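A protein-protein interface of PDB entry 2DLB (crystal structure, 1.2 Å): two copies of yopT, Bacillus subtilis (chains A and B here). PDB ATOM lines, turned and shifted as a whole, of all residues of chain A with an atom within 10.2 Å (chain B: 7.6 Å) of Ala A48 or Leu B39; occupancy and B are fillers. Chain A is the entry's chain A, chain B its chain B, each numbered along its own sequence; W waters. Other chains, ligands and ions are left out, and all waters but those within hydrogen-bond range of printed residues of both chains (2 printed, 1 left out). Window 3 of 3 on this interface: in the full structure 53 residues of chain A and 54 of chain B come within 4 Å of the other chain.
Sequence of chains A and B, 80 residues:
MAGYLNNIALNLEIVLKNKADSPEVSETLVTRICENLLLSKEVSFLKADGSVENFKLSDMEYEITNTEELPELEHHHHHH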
ATOM      1  N   LEU A  12      28.118   6.131  24.168  1.00  0.00           N
ATOM      2  CA  LEU A  12      27.230   7.252  24.117  1.00  0.00           C
ATOM      3  C   LEU A  12      27.572   8.262  25.213  1.00  0.00           C
ATOM      4  O   LEU A  12      28.036   7.895  26.266  1.00  0.00           O
ATOM      5  CB  LEU A  12      25.788   6.818  24.383  1.00  0.00           C
ATOM      6  CG  LEU A  12      25.294   5.616  23.563  1.00  0.00           C
ATOM      7  CD1 LEU A  12      23.810   5.397  23.857  1.00  0.00           C
ATOM      8  CD2 LEU A  12      25.550   5.764  22.099  1.00  0.00           C
ATOM      9  N   PHE A  45      16.936   4.170  19.375  1.00  0.00           N
ATOM     10  CA  PHE A  45      17.508   5.440  18.936  1.00  0.00           C
ATOM     11  C   PHE A  45      16.486   6.200  18.094  1.00  0.00           C
ATOM     12  O   PHE A  45      15.919   5.633  17.168  1.00  0.00           O
ATOM     13  CB  PHE A  45      18.774   5.241  18.116  1.00  0.00           C
ATOM     14  CG  PHE A  45      19.919   4.743  18.968  1.00  0.00           C
ATOM     15  CD1 PHE A  45      20.057   3.435  19.261  1.00  0.00           C
ATOM     16  CD2 PHE A  45      20.804   5.669  19.495  1.00  0.00           C
ATOM     17  CE1 PHE A  45      21.073   3.005  20.089  1.00  0.00           C
ATOM     18  CE2 PHE A  45      21.825   5.225  20.302  1.00  0.00           C
ATOM     19  CZ  PHE A  45      21.973   3.907  20.611  1.00  0.00           C
ATOM     20  N   LEU A  46      16.271   7.480  18.390  1.00  0.00           N
ATOM     21  CA  LEU A  46      15.526   8.427  17.582  1.00  0.00           C
ATOM     22  C   LEU A  46      16.541   9.032  16.608  1.00  0.00           C
ATOM     23  O   LEU A  46      17.348   9.900  16.964  1.00  0.00           O
ATOM     24  CB  LEU A  46      14.883   9.484  18.439  1.00  0.00           C
ATOM     25  CG  LEU A  46      14.137  10.594  17.666  1.00  0.00           C
ATOM     26  CD1 LEU A  46      13.034  10.040  16.804  1.00  0.00           C
ATOM     27  CD2 LEU A  46      13.599  11.593  18.685  1.00  0.00           C
ATOM     28  N   LYS A  47      16.554   8.520  15.367  1.00  0.00           N
ATOM     29  CA  LYS A  47      17.563   8.869  14.380  1.00  0.00           C
ATOM     30  C   LYS A  47      17.287  10.255  13.836  1.00  0.00           C
ATOM     31  O   LYS A  47      16.233  10.859  14.053  1.00  0.00           O
ATOM     32  CB  LYS A  47      17.580   7.766  13.312  1.00  0.00           C
ATOM     33  CG  LYS A  47      18.060   6.435  13.810  1.00  0.00           C
ATOM     34  CD  LYS A  47      18.029   5.244  12.882  1.00  0.00           C
ATOM     35  CE  LYS A  47      16.672   4.753  12.495  1.00  0.00           C
ATOM     36  NZ  LYS A  47      16.827   3.551  11.572  1.00  0.00           N
ATOM     37  N   ALA A  48      18.279  10.781  13.132  1.00  0.00           N
ATOM     38  CA  ALA A  48      18.211  12.143  12.610  1.00  0.00           C
ATOM     39  C   ALA A  48      16.980  12.325  11.736  1.00  0.00           C
ATOM     40  O   ALA A  48      16.413  13.428  11.751  1.00  0.00           O
ATOM     41  CB  ALA A  48      19.458  12.505  11.831  1.00  0.00           C
ATOM     42  N   ASP A  49      16.560  11.343  10.970  1.00  0.00           N
ATOM     43  CA  ASP A  49      15.409  11.466  10.107  1.00  0.00           C
ATOM     44  C   ASP A  49      14.079  11.266  10.845  1.00  0.00           C
ATOM     45  O   ASP A  49      13.014  11.353  10.214  1.00  0.00           O
ATOM     46  CB  ASP A  49      15.475  10.499   8.944  1.00  0.00           C
ATOM     47  CG  ASP A  49      15.508   9.024   9.284  1.00  0.00           C
ATOM     48  OD1 ASP A  49      15.274   8.681  10.434  1.00  0.00           O
ATOM     49  OD2 ASP A  49      15.719   8.216   8.326  1.00  0.00           O
ATOM     50  N   GLY A  50      14.112  11.064  12.158  1.00  0.00           N
ATOM     51  CA  GLY A  50      12.903  10.914  12.939  1.00  0.00           C
ATOM     52  C   GLY A  50      12.407   9.509  13.114  1.00  0.00           C
ATOM     53  O   GLY A  50      11.459   9.300  13.887  1.00  0.00           O
ATOM     54  N   SER A  51      13.019   8.545  12.418  1.00  0.00           N
ATOM     55  CA  SER A  51      12.637   7.165  12.626  1.00  0.00           C
ATOM     56  C   SER A  51      13.284   6.617  13.892  1.00  0.00           C
ATOM     57  O   SER A  51      14.312   7.116  14.298  1.00  0.00           O
ATOM     58  CB  SER A  51      13.029   6.344  11.409  1.00  0.00           C
ATOM     59  OG  SER A  51      14.406   6.182  11.273  1.00  0.00           O
ATOM     60  N   VAL A  52      12.653   5.620  14.467  1.00  0.00           N
ATOM     61  CA  VAL A  52      13.137   4.990  15.702  1.00  0.00           C
ATOM     62  C   VAL A  52      13.563   3.582  15.386  1.00  0.00           C
ATOM     63  O   VAL A  52      12.807   2.827  14.746  1.00  0.00           O
ATOM     64  CB  VAL A  52      12.046   5.041  16.775  1.00  0.00           C
ATOM     65  CG1 VAL A  52      12.506   4.206  17.970  1.00  0.00           C
ATOM     66  CG2 VAL A  52      11.721   6.493  17.124  1.00  0.00           C
ATOM     67  N   GLU A  53      14.743   3.210  15.823  1.00  0.00           N
ATOM     68  CA  GLU A  53      15.242   1.855  15.631  1.00  0.00           C
ATOM     69  C   GLU A  53      15.538   1.220  16.999  1.00  0.00           C
ATOM     70  O   GLU A  53      16.229   1.828  17.824  1.00  0.00           O
ATOM     71  CB  GLU A  53      16.471   1.829  14.747  1.00  0.00           C
ATOM     72  CG  GLU A  53      16.937   0.443  14.368  1.00  0.00           C
ATOM     73  CD  GLU A  53      18.055   0.349  13.358  1.00  0.00           C
ATOM     74  OE1 GLU A  53      18.517   1.432  12.928  1.00  0.00           O
ATOM     75  OE2 GLU A  53      18.470  -0.799  13.048  1.00  0.00           O
ATOM     76  N   CYS B  34      25.003   1.223  11.910  1.00  0.00           N
ATOM     77  CA  CYS B  34      25.542   2.034  12.989  1.00  0.00           C
ATOM     78  C   CYS B  34      25.878   3.436  12.550  1.00  0.00           C
ATOM     79  O   CYS B  34      25.697   4.384  13.324  1.00  0.00           O
ATOM     80  CB  CYS B  34      26.786   1.341  13.604  1.00  0.00           C
ATOM     81  SG  CYS B  34      26.303  -0.171  14.486  1.00  0.00           S
ATOM     82  N   GLU B  35      26.390   3.627  11.348  1.00  0.00           N
ATOM     83  CA  GLU B  35      26.638   4.972  10.825  1.00  0.00           C
ATOM     84  C   GLU B  35      25.369   5.823  10.830  1.00  0.00           C
ATOM     85  O   GLU B  35      25.452   7.029  11.060  1.00  0.00           O
ATOM     86  CB  GLU B  35      27.234   4.885   9.419  1.00  0.00           C
ATOM     87  CG  GLU B  35      28.685   4.484   9.341  1.00  0.00           C
ATOM     88  CD  GLU B  35      29.612   5.526   9.904  1.00  0.00           C
ATOM     89  OE1 GLU B  35      30.268   5.198  10.902  1.00  0.00           O
ATOM     90  OE2 GLU B  35      29.663   6.622   9.324  1.00  0.00           O
ATOM     91  N   ASN B  36      24.252   5.172  10.572  1.00  0.00           N
ATOM     92  CA  ASN B  36      22.981   5.850  10.565  1.00  0.00           C
ATOM     93  C   ASN B  36      22.396   6.127  11.931  1.00  0.00           C
ATOM     94  O   ASN B  36      21.334   6.722  12.068  1.00  0.00           O
ATOM     95  CB  ASN B  36      22.021   5.020   9.701  1.00  0.00           C
ATOM     96  CG  ASN B  36      22.203   5.141   8.220  1.00  0.00           C
ATOM     97  OD1 ASN B  36      22.738   6.166   7.780  1.00  0.00           O
ATOM     98  ND2 ASN B  36      21.774   4.160   7.443  1.00  0.00           N
ATOM     99  N   LEU B  37      23.110   5.709  13.001  1.00  0.00           N
ATOM    100  CA  LEU B  37      22.732   6.104  14.370  1.00  0.00           C
ATOM    101  C   LEU B  37      23.498   7.330  14.835  1.00  0.00           C
ATOM    102  O   LEU B  37      23.030   7.942  15.795  1.00  0.00           O
ATOM    103  CB  LEU B  37      23.039   4.960  15.329  1.00  0.00           C
ATOM    104  CG  LEU B  37      22.362   3.644  15.061  1.00  0.00           C
ATOM    105  CD1 LEU B  37      22.820   2.648  16.127  1.00  0.00           C
ATOM    106  CD2 LEU B  37      20.837   3.766  15.048  1.00  0.00           C
ATOM    107  N   LEU B  38      24.616   7.692  14.229  1.00  0.00           N
ATOM    108  CA  LEU B  38      25.505   8.708  14.812  1.00  0.00           C
ATOM    109  C   LEU B  38      24.977  10.044  15.207  1.00  0.00           C
ATOM    110  O   LEU B  38      25.411  10.696  16.193  1.00  0.00           O
ATOM    111  CB  LEU B  38      26.674   8.934  13.803  1.00  0.00           C
ATOM    112  CG  LEU B  38      27.658   7.761  13.797  1.00  0.00           C
ATOM    113  CD1 LEU B  38      28.744   8.050  12.748  1.00  0.00           C
ATOM    114  CD2 LEU B  38      28.389   7.524  15.098  1.00  0.00           C
ATOM    115  N   LEU B  39      24.004  10.504  14.438  1.00  0.00           N
ATOM    116  CA  LEU B  39      23.397  11.833  14.674  1.00  0.00           C
ATOM    117  C   LEU B  39      22.012  11.735  15.293  1.00  0.00           C
ATOM    118  O   LEU B  39      21.174  12.636  15.269  1.00  0.00           O
ATOM    119  CB  LEU B  39      23.352  12.576  13.351  1.00  0.00           C
ATOM    120  CG  LEU B  39      24.723  12.812  12.710  1.00  0.00           C
ATOM    121  CD1 LEU B  39      24.519  13.346  11.318  1.00  0.00           C
ATOM    122  CD2 LEU B  39      25.555  13.727  13.616  1.00  0.00           C
ATOM    123  N   SER B  40      21.755  10.621  15.967  1.00  0.00           N
ATOM    124  CA  SER B  40      20.520  10.485  16.717  1.00  0.00           C
ATOM    125  C   SER B  40      20.413  11.565  17.788  1.00  0.00           C
ATOM    126  O   SER B  40      21.377  11.963  18.413  1.00  0.00           O
ATOM    127  CB  SER B  40      20.418   9.129  17.369  1.00  0.00           C
ATOM    128  OG  SER B  40      20.322   8.084  16.437  1.00  0.00           O
ATOM    129  N   LYS B  41      19.186  12.026  18.059  1.00  0.00           N
ATOM    130  CA  LYS B  41      18.968  13.007  19.076  1.00  0.00           C
ATOM    131  C   LYS B  41      18.600  12.460  20.450  1.00  0.00           C
ATOM    132  O   LYS B  41      18.812  13.165  21.455  1.00  0.00           O
ATOM    133  CB  LYS B  41      17.838  13.971  18.615  1.00  0.00           C
ATOM    134  CG  LYS B  41      18.271  14.852  17.465  1.00  0.00           C
ATOM    135  CD  LYS B  41      19.408  15.818  17.686  1.00  0.00           C
ATOM    136  CE  LYS B  41      20.298  15.999  16.480  1.00  0.00           C
ATOM    137  NZ  LYS B  41      21.290  14.903  16.303  1.00  0.00           N
ATOM    138  N   GLU B  42      18.081  11.254  20.506  1.00  0.00           N
ATOM    139  CA  GLU B  42      17.603  10.660  21.756  1.00  0.00           C
ATOM    140  C   GLU B  42      17.919   9.174  21.736  1.00  0.00           C
ATOM    141  O   GLU B  42      17.917   8.542  20.689  1.00  0.00           O
ATOM    142  CB  GLU B  42      16.091  10.834  21.925  1.00  0.00           C
ATOM    143  CG  GLU B  42      15.339  10.329  23.127  1.00  0.00           C
ATOM    144  CD  GLU B  42      13.853  10.587  22.912  1.00  0.00           C
ATOM    145  OE1 GLU B  42      13.031   9.657  22.825  1.00  0.00           O
ATOM    146  OE2 GLU B  42      13.625  11.812  22.854  1.00  0.00           O
ATOM    147  N   LEU B  57      20.849  12.738  23.639  1.00  0.00           N
ATOM    148  CA  LEU B  57      22.167  12.269  23.242  1.00  0.00           C
ATOM    149  C   LEU B  57      23.025  13.451  22.806  1.00  0.00           C
ATOM    150  O   LEU B  57      22.563  14.241  22.004  1.00  0.00           O
ATOM    151  CB  LEU B  57      21.965  11.299  22.123  1.00  0.00           C
ATOM    152  CG  LEU B  57      22.857  10.215  21.696  1.00  0.00           C
ATOM    153  CD1 LEU B  57      23.496   9.448  22.830  1.00  0.00           C
ATOM    154  CD2 LEU B  57      21.956   9.378  20.785  1.00  0.00           C
ATOM    155  N   MET B  60      28.103  10.123  20.118  1.00  0.00           N
ATOM    156  CA  MET B  60      28.182   8.698  19.967  1.00  0.00           C
ATOM    157  C   MET B  60      29.389   8.253  19.161  1.00  0.00           C
ATOM    158  O   MET B  60      29.728   8.915  18.192  1.00  0.00           O
ATOM    159  CB  MET B  60      26.901   8.274  19.238  1.00  0.00           C
ATOM    160  CG  MET B  60      26.854   6.847  18.842  1.00  0.00           C
ATOM    161  SD  MET B  60      25.227   6.407  18.058  1.00  0.00           S
ATOM    162  CE  MET B  60      24.211   8.018  18.314  1.00  0.00           C
HETATM  163  O   HOH W   1      20.751   9.344  12.731  1.00  0.00           O
HETATM  164  O   HOH W   2      14.690   7.019  21.391  1.00  0.00           O
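Of the printed residues of chain B, Leu A12 touches Leu B57 and Met B60.
Printed residues of chain B within 4 Å of Leu A46: Ser B40 (3.2 Å), Lys B41 (3.0 Å) and Glu B42 (3.0 Å).
Of the printed residues of chain B, Lys A47 touches Asn B36 (3.7 Å), Leu B37 (3.8 Å) and Ser B40 (3.5 Å).
Of chain B, only Leu B39 comes within 4 Å of Ala A48.
Glu B35 touches none of the printed residues of chain A.
Of the printed residues of chain A, Leu B37 touches Phe A45, Lys A47 and Glu A53.
Of the printed residues of chain A, Leu B39 touches Ala A48 (3.8 Å).
The nearest residue of chain A that does not touch Leu B39 is Lys A47 (4.8 Å).
The nearest printed residue of chain A that does not touch Leu B37 is Leu A46 (6.1 Å).
Among the printed residues, merely in contact across the chains: Leu A46 with Ser B40, Lys A47 with Ser B40, Phe A45 with Glu B42, Phe A45 with Ser B40, Leu A12 with Met B60, Lys A47 with Asn B36, Leu A12 with Leu B57, Lys A47 with Leu B37, Ala A48 with Leu B39, Glu A53 with Leu B37 and Phe A45 with Leu B37.
Among the printed residues, 13 pairs touch across the chains.
The backbone carbonyl oxygen of Glu B42 sits at hydrogen-bond distance from the backbone NH of Leu A46.
The backbone carbonyl oxygen (O) of Leu A46 lies within hydrogen-bond range of the backbone NH (N) of Lys B41 (3.0 Å).
The backbone NH (N) of Leu B57 is in hydrogen-bond range of the backbone carbonyl oxygen (O) of Lys B41.
O of Leu B37 is in hydrogen-bond range of OG of Ser B40, at 2.8 Å.
O of Leu B39 is in hydrogen-bond range of NZ of Lys B41 (2.5 Å).
O of Glu A53 lies within hydrogen-bond range of N of Phe A45 (2.9 Å).
NZ of Lys A47 lies within salt-bridge range of OE1 of Glu A53 (3.0 Å).
No position is printed for both chains.
Water W1 bridges the backbone carbonyl oxygen (O) of Asn B36 (2.8 Å) and the backbone NH (N) of Ala A48 (2.9 Å).
Water W2 lies within hydrogen-bond range of N of Leu A46 (3.4 Å) and OE1 of Glu B42 (3.4 Å).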
